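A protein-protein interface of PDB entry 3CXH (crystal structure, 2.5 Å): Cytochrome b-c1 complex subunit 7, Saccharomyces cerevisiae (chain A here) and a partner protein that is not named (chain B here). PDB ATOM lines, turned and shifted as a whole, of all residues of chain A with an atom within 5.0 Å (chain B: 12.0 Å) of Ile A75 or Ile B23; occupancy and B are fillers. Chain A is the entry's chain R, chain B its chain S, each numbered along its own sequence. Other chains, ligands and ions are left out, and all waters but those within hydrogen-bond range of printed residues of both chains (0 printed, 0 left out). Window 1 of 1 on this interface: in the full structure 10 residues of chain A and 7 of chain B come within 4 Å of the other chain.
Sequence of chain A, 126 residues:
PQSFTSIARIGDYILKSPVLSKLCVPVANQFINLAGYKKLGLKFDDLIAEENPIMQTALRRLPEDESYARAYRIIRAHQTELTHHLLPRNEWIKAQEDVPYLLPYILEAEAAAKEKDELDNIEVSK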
ATOM      1  N   TYR A  68       7.027 -21.784 -24.397  1.00  0.00           N
ATOM      2  CA  TYR A  68       8.477 -21.730 -24.528  1.00  0.00           C
ATOM      3  C   TYR A  68       9.071 -21.385 -23.171  1.00  0.00           C
ATOM      4  O   TYR A  68      10.154 -21.856 -22.802  1.00  0.00           O
ATOM      5  CB  TYR A  68       8.892 -20.664 -25.543  1.00  0.00           C
ATOM      6  CG  TYR A  68       8.501 -20.959 -26.974  1.00  0.00           C
ATOM      7  CD1 TYR A  68       8.081 -19.930 -27.831  1.00  0.00           C
ATOM      8  CD2 TYR A  68       8.542 -22.264 -27.475  1.00  0.00           C
ATOM      9  CE1 TYR A  68       7.708 -20.200 -29.152  1.00  0.00           C
ATOM     10  CE2 TYR A  68       8.172 -22.543 -28.783  1.00  0.00           C
ATOM     11  CZ  TYR A  68       7.755 -21.512 -29.614  1.00  0.00           C
ATOM     12  OH  TYR A  68       7.367 -21.802 -30.897  1.00  0.00           O
ATOM     13  N   ALA A  71       8.995 -24.531 -20.953  1.00  0.00           N
ATOM     14  CA  ALA A  71      10.065 -25.423 -21.351  1.00  0.00           C
ATOM     15  C   ALA A  71      11.401 -25.005 -20.737  1.00  0.00           C
ATOM     16  O   ALA A  71      12.159 -25.851 -20.250  1.00  0.00           O
ATOM     17  CB  ALA A  71      10.170 -25.462 -22.863  1.00  0.00           C
ATOM     18  N   TYR A  72      11.674 -23.706 -20.730  1.00  0.00           N
ATOM     19  CA  TYR A  72      12.928 -23.225 -20.174  1.00  0.00           C
ATOM     20  C   TYR A  72      13.043 -23.510 -18.679  1.00  0.00           C
ATOM     21  O   TYR A  72      14.081 -23.974 -18.204  1.00  0.00           O
ATOM     22  CB  TYR A  72      13.096 -21.721 -20.418  1.00  0.00           C
ATOM     23  CG  TYR A  72      14.336 -21.171 -19.761  1.00  0.00           C
ATOM     24  CD1 TYR A  72      15.597 -21.611 -20.153  1.00  0.00           C
ATOM     25  CD2 TYR A  72      14.249 -20.263 -18.695  1.00  0.00           C
ATOM     26  CE1 TYR A  72      16.737 -21.176 -19.506  1.00  0.00           C
ATOM     27  CE2 TYR A  72      15.397 -19.817 -18.033  1.00  0.00           C
ATOM     28  CZ  TYR A  72      16.634 -20.284 -18.448  1.00  0.00           C
ATOM     29  OH  TYR A  72      17.785 -19.893 -17.803  1.00  0.00           O
ATOM     30  N   ARG A  73      11.970 -23.243 -17.944  1.00  0.00           N
ATOM     31  CA  ARG A  73      11.983 -23.441 -16.508  1.00  0.00           C
ATOM     32  C   ARG A  73      12.196 -24.893 -16.145  1.00  0.00           C
ATOM     33  O   ARG A  73      12.853 -25.206 -15.152  1.00  0.00           O
ATOM     34  CB  ARG A  73      10.696 -22.909 -15.890  1.00  0.00           C
ATOM     35  CG  ARG A  73      10.516 -21.406 -16.033  1.00  0.00           C
ATOM     36  CD  ARG A  73       9.418 -20.901 -15.106  1.00  0.00           C
ATOM     37  NE  ARG A  73       8.111 -21.500 -15.371  1.00  0.00           N
ATOM     38  CZ  ARG A  73       7.230 -21.044 -16.264  1.00  0.00           C
ATOM     39  NH1 ARG A  73       6.063 -21.667 -16.414  1.00  0.00           N
ATOM     40  NH2 ARG A  73       7.503 -19.972 -17.006  1.00  0.00           N
ATOM     41  N   ILE A  74      11.654 -25.779 -16.974  1.00  0.00           N
ATOM     42  CA  ILE A  74      11.783 -27.200 -16.764  1.00  0.00           C
ATOM     43  C   ILE A  74      13.221 -27.637 -17.042  1.00  0.00           C
ATOM     44  O   ILE A  74      13.856 -28.277 -16.200  1.00  0.00           O
ATOM     45  CB  ILE A  74      10.778 -27.960 -17.649  1.00  0.00           C
ATOM     46  CG1 ILE A  74       9.360 -27.654 -17.148  1.00  0.00           C
ATOM     47  CG2 ILE A  74      11.092 -29.473 -17.672  1.00  0.00           C
ATOM     48  CD1 ILE A  74       8.268 -28.420 -17.842  1.00  0.00           C
ATOM     49  N   ILE A  75      13.754 -27.248 -18.196  1.00  0.00           N
ATOM     50  CA  ILE A  75      15.121 -27.623 -18.540  1.00  0.00           C
ATOM     51  C   ILE A  75      16.114 -27.073 -17.519  1.00  0.00           C
ATOM     52  O   ILE A  75      16.956 -27.806 -17.008  1.00  0.00           O
ATOM     53  CB  ILE A  75      15.504 -27.156 -19.958  1.00  0.00           C
ATOM     54  CG1 ILE A  75      14.593 -27.833 -20.999  1.00  0.00           C
ATOM     55  CG2 ILE A  75      16.971 -27.491 -20.250  1.00  0.00           C
ATOM     56  CD1 ILE A  75      14.793 -27.322 -22.430  1.00  0.00           C
ATOM     57  N   ARG A  76      15.955 -25.806 -17.166  1.00  0.00           N
ATOM     58  CA  ARG A  76      16.837 -25.161 -16.206  1.00  0.00           C
ATOM     59  C   ARG A  76      16.774 -25.873 -14.847  1.00  0.00           C
ATOM     60  O   ARG A  76      17.791 -26.067 -14.187  1.00  0.00           O
ATOM     61  CB  ARG A  76      16.459 -23.675 -16.099  1.00  0.00           C
ATOM     62  CG  ARG A  76      17.190 -22.872 -15.045  1.00  0.00           C
ATOM     63  CD  ARG A  76      16.181 -22.121 -14.205  1.00  0.00           C
ATOM     64  NE  ARG A  76      16.094 -20.710 -14.548  1.00  0.00           N
ATOM     65  CZ  ARG A  76      15.058 -19.923 -14.269  1.00  0.00           C
ATOM     66  NH1 ARG A  76      15.106 -18.648 -14.617  1.00  0.00           N
ATOM     67  NH2 ARG A  76      13.964 -20.408 -13.697  1.00  0.00           N
ATOM     68  N   ALA A  77      15.589 -26.328 -14.470  1.00  0.00           N
ATOM     69  CA  ALA A  77      15.420 -27.043 -13.207  1.00  0.00           C
ATOM     70  C   ALA A  77      16.148 -28.397 -13.177  1.00  0.00           C
ATOM     71  O   ALA A  77      16.840 -28.692 -12.198  1.00  0.00           O
ATOM     72  CB  ALA A  77      13.945 -27.232 -12.893  1.00  0.00           C
ATOM     73  N   HIS A  78      15.981 -29.220 -14.222  1.00  0.00           N
ATOM     74  CA  HIS A  78      16.658 -30.526 -14.275  1.00  0.00           C
ATOM     75  C   HIS A  78      18.172 -30.337 -14.166  1.00  0.00           C
ATOM     76  O   HIS A  78      18.850 -31.104 -13.490  1.00  0.00           O
ATOM     77  CB  HIS A  78      16.329 -31.310 -15.569  1.00  0.00           C
ATOM     78  CG  HIS A  78      14.967 -31.936 -15.574  1.00  0.00           C
ATOM     79  ND1 HIS A  78      13.958 -31.522 -16.418  1.00  0.00           N
ATOM     80  CD2 HIS A  78      14.428 -32.902 -14.796  1.00  0.00           C
ATOM     81  CE1 HIS A  78      12.854 -32.196 -16.150  1.00  0.00           C
ATOM     82  NE2 HIS A  78      13.113 -33.040 -15.168  1.00  0.00           N
ATOM     83  N   GLN A  79      18.688 -29.305 -14.828  1.00  0.00           N
ATOM     84  CA  GLN A  79      20.116 -29.015 -14.805  1.00  0.00           C
ATOM     85  C   GLN A  79      20.555 -28.620 -13.398  1.00  0.00           C
ATOM     86  O   GLN A  79      21.523 -29.169 -12.858  1.00  0.00           O
ATOM     87  CB  GLN A  79      20.457 -27.909 -15.800  1.00  0.00           C
ATOM     88  CG  GLN A  79      21.932 -27.517 -15.825  1.00  0.00           C
ATOM     89  CD  GLN A  79      22.860 -28.632 -16.290  1.00  0.00           C
ATOM     90  OE1 GLN A  79      22.512 -29.433 -17.155  1.00  0.00           O
ATOM     91  NE2 GLN A  79      24.058 -28.668 -15.729  1.00  0.00           N
ATOM     92  N   TRP B  12      14.890 -40.181 -29.827  1.00  0.00           N
ATOM     93  CA  TRP B  12      15.715 -39.116 -30.400  1.00  0.00           C
ATOM     94  C   TRP B  12      15.162 -38.544 -31.700  1.00  0.00           C
ATOM     95  O   TRP B  12      15.081 -39.238 -32.712  1.00  0.00           O
ATOM     96  CB  TRP B  12      17.139 -39.630 -30.641  1.00  0.00           C
ATOM     97  CG  TRP B  12      17.836 -40.078 -29.386  1.00  0.00           C
ATOM     98  CD1 TRP B  12      18.202 -41.356 -29.062  1.00  0.00           C
ATOM     99  CD2 TRP B  12      18.236 -39.251 -28.282  1.00  0.00           C
ATOM    100  NE1 TRP B  12      18.800 -41.376 -27.821  1.00  0.00           N
ATOM    101  CE2 TRP B  12      18.829 -40.100 -27.317  1.00  0.00           C
ATOM    102  CE3 TRP B  12      18.151 -37.875 -28.015  1.00  0.00           C
ATOM    103  CZ2 TRP B  12      19.332 -39.617 -26.098  1.00  0.00           C
ATOM    104  CZ3 TRP B  12      18.652 -37.393 -26.804  1.00  0.00           C
ATOM    105  CH2 TRP B  12      19.233 -38.262 -25.862  1.00  0.00           C
ATOM    106  N   MET B  15      11.065 -36.907 -29.230  1.00  0.00           N
ATOM    107  CA  MET B  15      10.955 -37.323 -27.837  1.00  0.00           C
ATOM    108  C   MET B  15       9.571 -37.235 -27.200  1.00  0.00           C
ATOM    109  O   MET B  15       9.263 -38.012 -26.283  1.00  0.00           O
ATOM    110  CB  MET B  15      11.962 -36.560 -26.991  1.00  0.00           C
ATOM    111  CG  MET B  15      12.336 -37.249 -25.693  1.00  0.00           C
ATOM    112  SD  MET B  15      13.168 -38.801 -25.973  1.00  0.00           S
ATOM    113  CE  MET B  15      14.776 -38.258 -26.653  1.00  0.00           C
ATOM    114  N   GLY B  16       8.762 -36.275 -27.652  1.00  0.00           N
ATOM    115  CA  GLY B  16       7.425 -36.117 -27.114  1.00  0.00           C
ATOM    116  C   GLY B  16       7.207 -34.843 -26.316  1.00  0.00           C
ATOM    117  O   GLY B  16       6.149 -34.642 -25.713  1.00  0.00           O
ATOM    118  N   GLY B  17       8.202 -33.968 -26.307  1.00  0.00           N
ATOM    119  CA  GLY B  17       8.069 -32.735 -25.559  1.00  0.00           C
ATOM    120  C   GLY B  17       7.543 -31.599 -26.400  1.00  0.00           C
ATOM    121  O   GLY B  17       7.292 -31.761 -27.597  1.00  0.00           O
ATOM    122  N   PRO B  18       7.349 -30.427 -25.792  1.00  0.00           N
ATOM    123  CA  PRO B  18       6.852 -29.271 -26.522  1.00  0.00           C
ATOM    124  C   PRO B  18       7.959 -28.745 -27.426  1.00  0.00           C
ATOM    125  O   PRO B  18       9.118 -29.133 -27.276  1.00  0.00           O
ATOM    126  CB  PRO B  18       6.539 -28.287 -25.404  1.00  0.00           C
ATOM    127  CG  PRO B  18       7.595 -28.580 -24.406  1.00  0.00           C
ATOM    128  CD  PRO B  18       7.588 -30.095 -24.378  1.00  0.00           C
ATOM    129  N   LYS B  19       7.601 -27.893 -28.382  1.00  0.00           N
ATOM    130  CA  LYS B  19       8.594 -27.322 -29.277  1.00  0.00           C
ATOM    131  C   LYS B  19       9.496 -26.380 -28.483  1.00  0.00           C
ATOM    132  O   LYS B  19       9.035 -25.639 -27.624  1.00  0.00           O
ATOM    133  CB  LYS B  19       7.916 -26.590 -30.439  1.00  0.00           C
ATOM    134  CG  LYS B  19       7.032 -27.489 -31.273  1.00  0.00           C
ATOM    135  CD  LYS B  19       6.748 -26.924 -32.656  1.00  0.00           C
ATOM    136  CE  LYS B  19       5.721 -27.792 -33.390  1.00  0.00           C
ATOM    137  NZ  LYS B  19       5.985 -29.258 -33.184  1.00  0.00           N
ATOM    138  N   GLN B  20      10.794 -26.449 -28.737  1.00  0.00           N
ATOM    139  CA  GLN B  20      11.746 -25.604 -28.023  1.00  0.00           C
ATOM    140  C   GLN B  20      12.313 -24.507 -28.909  1.00  0.00           C
ATOM    141  O   GLN B  20      12.835 -24.784 -29.992  1.00  0.00           O
ATOM    142  CB  GLN B  20      12.881 -26.454 -27.454  1.00  0.00           C
ATOM    143  CG  GLN B  20      12.422 -27.501 -26.455  1.00  0.00           C
ATOM    144  CD  GLN B  20      13.576 -28.296 -25.920  1.00  0.00           C
ATOM    145  OE1 GLN B  20      14.720 -27.818 -25.909  1.00  0.00           O
ATOM    146  NE2 GLN B  20      13.301 -29.523 -25.479  1.00  0.00           N
ATOM    147  N   LYS B  21      12.228 -23.272 -28.424  1.00  0.00           N
ATOM    148  CA  LYS B  21      12.718 -22.101 -29.145  1.00  0.00           C
ATOM    149  C   LYS B  21      13.221 -21.040 -28.146  1.00  0.00           C
ATOM    150  O   LYS B  21      12.611 -20.825 -27.093  1.00  0.00           O
ATOM    151  CB  LYS B  21      11.571 -21.521 -29.981  1.00  0.00           C
ATOM    152  CG  LYS B  21      11.961 -20.702 -31.207  1.00  0.00           C
ATOM    153  CD  LYS B  21      10.714 -20.003 -31.748  1.00  0.00           C
ATOM    154  CE  LYS B  21      10.842 -19.537 -33.206  1.00  0.00           C
ATOM    155  NZ  LYS B  21      12.045 -18.729 -33.433  1.00  0.00           N
ATOM    156  N   GLY B  22      14.347 -20.402 -28.466  1.00  0.00           N
ATOM    157  CA  GLY B  22      14.889 -19.359 -27.608  1.00  0.00           C
ATOM    158  C   GLY B  22      15.883 -19.775 -26.544  1.00  0.00           C
ATOM    159  O   GLY B  22      16.478 -18.918 -25.878  1.00  0.00           O
ATOM    160  N   ILE B  23      16.032 -21.080 -26.333  1.00  0.00           N
ATOM    161  CA  ILE B  23      16.985 -21.558 -25.346  1.00  0.00           C
ATOM    162  C   ILE B  23      18.285 -21.888 -26.042  1.00  0.00           C
ATOM    163  O   ILE B  23      18.298 -22.560 -27.067  1.00  0.00           O
ATOM    164  CB  ILE B  23      16.503 -22.827 -24.639  1.00  0.00           C
ATOM    165  CG1 ILE B  23      15.116 -22.608 -24.046  1.00  0.00           C
ATOM    166  CG2 ILE B  23      17.493 -23.230 -23.538  1.00  0.00           C
ATOM    167  CD1 ILE B  23      14.561 -23.851 -23.409  1.00  0.00           C
ATOM    168  N   THR B  24      19.376 -21.358 -25.516  1.00  0.00           N
ATOM    169  CA  THR B  24      20.692 -21.637 -26.069  1.00  0.00           C
ATOM    170  C   THR B  24      21.469 -22.299 -24.949  1.00  0.00           C
ATOM    171  O   THR B  24      21.350 -21.906 -23.790  1.00  0.00           O
ATOM    172  CB  THR B  24      21.430 -20.347 -26.476  1.00  0.00           C
ATOM    173  OG1 THR B  24      20.668 -19.657 -27.476  1.00  0.00           O
ATOM    174  CG2 THR B  24      22.823 -20.675 -27.021  1.00  0.00           C
ATOM    175  N   SER B  25      22.220 -23.340 -25.274  1.00  0.00           N
ATOM    176  CA  SER B  25      23.006 -24.013 -24.256  1.00  0.00           C
ATOM    177  C   SER B  25      24.475 -24.033 -24.673  1.00  0.00           C
ATOM    178  O   SER B  25      24.801 -23.986 -25.860  1.00  0.00           O
ATOM    179  CB  SER B  25      22.479 -25.432 -24.015  1.00  0.00           C
ATOM    180  OG  SER B  25      22.665 -26.249 -25.156  1.00  0.00           O
ATOM    181  N   TYR B  26      25.356 -24.090 -23.684  1.00  0.00           N
ATOM    182  CA  TYR B  26      26.792 -24.103 -23.935  1.00  0.00           C
ATOM    183  C   TYR B  26      27.404 -25.167 -23.057  1.00  0.00           C
ATOM    184  O   TYR B  26      26.911 -25.441 -21.963  1.00  0.00           O
ATOM    185  CB  TYR B  26      27.424 -22.748 -23.571  1.00  0.00           C
ATOM    186  CG  TYR B  26      26.796 -21.552 -24.249  1.00  0.00           C
ATOM    187  CD1 TYR B  26      25.620 -20.986 -23.763  1.00  0.00           C
ATOM    188  CD2 TYR B  26      27.382 -20.977 -25.379  1.00  0.00           C
ATOM    189  CE1 TYR B  26      25.041 -19.877 -24.388  1.00  0.00           C
ATOM    190  CE2 TYR B  26      26.807 -19.865 -26.010  1.00  0.00           C
ATOM    191  CZ  TYR B  26      25.642 -19.328 -25.508  1.00  0.00           C
ATOM    192  OH  TYR B  26      25.065 -18.249 -26.130  1.00  0.00           O
ATOM    193  N   ALA B  27      28.493 -25.747 -23.536  1.00  0.00           N
ATOM    194  CA  ALA B  27      29.205 -26.769 -22.795  1.00  0.00           C
ATOM    195  C   ALA B  27      30.659 -26.715 -23.222  1.00  0.00           C
ATOM    196  O   ALA B  27      30.984 -26.211 -24.297  1.00  0.00           O
ATOM    197  CB  ALA B  27      28.615 -28.155 -23.087  1.00  0.00           C
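Of the printed residues of chain B, Tyr A68 touches Lys B19 (3.4 Å) and Lys B21 (3.7 Å). No residue of chain B comes within 4 Å of Ala A71. Of chain B, only Ile B23 comes within 4 Å of Tyr A72. Arg A73 touches none of the printed residues of chain B. No residue of chain B comes within 4 Å of Ile A74. No residue of chain B comes within 4 Å of Ala A77. No residue of chain B comes within 4 Å of His A78. No residue of chain B comes within 4 Å of Gln A79. Pro B18 touches none of the printed residues of chain A. Printed residues of chain A within 4 Å of Gln B20: Ile A75 (3.5 Å). Of the printed residues of chain A, Lys B21 touches Tyr A68 (3.7 Å). Ile B23 touches two residues of chain A. The nearest residue of chain B that does not touch Ile A75 is Ser B25 (7.0 Å). The nearest printed residue of chain A that does not touch Gln B20 is Tyr A68 (4.6 Å).
Printed residues of chain B that touch a printed residue of chain A: Lys B19, Gln B20, Lys B21 and Ile B23. Hydrophobic or aromatic side chains of chain B within 4 Å of the printed part of chain A: Ile B23. Printed residues of chain A that touch a printed residue of chain B: Tyr A68, Tyr A72 and Ile A75. Among the printed residues, 5 pairs touch across the chains. Among the printed residues, no Asp or Glu carboxylate lies within 4 Å of a Lys or Arg side-chain nitrogen of the other chain.
Among the printed residues, merely in contact across the chains: Tyr A68 with Lys B19, Ile A75 with Gln B20, Ile A75 with Ile B23, Tyr A72 with Ile B23 and Tyr A68 with Lys B21.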
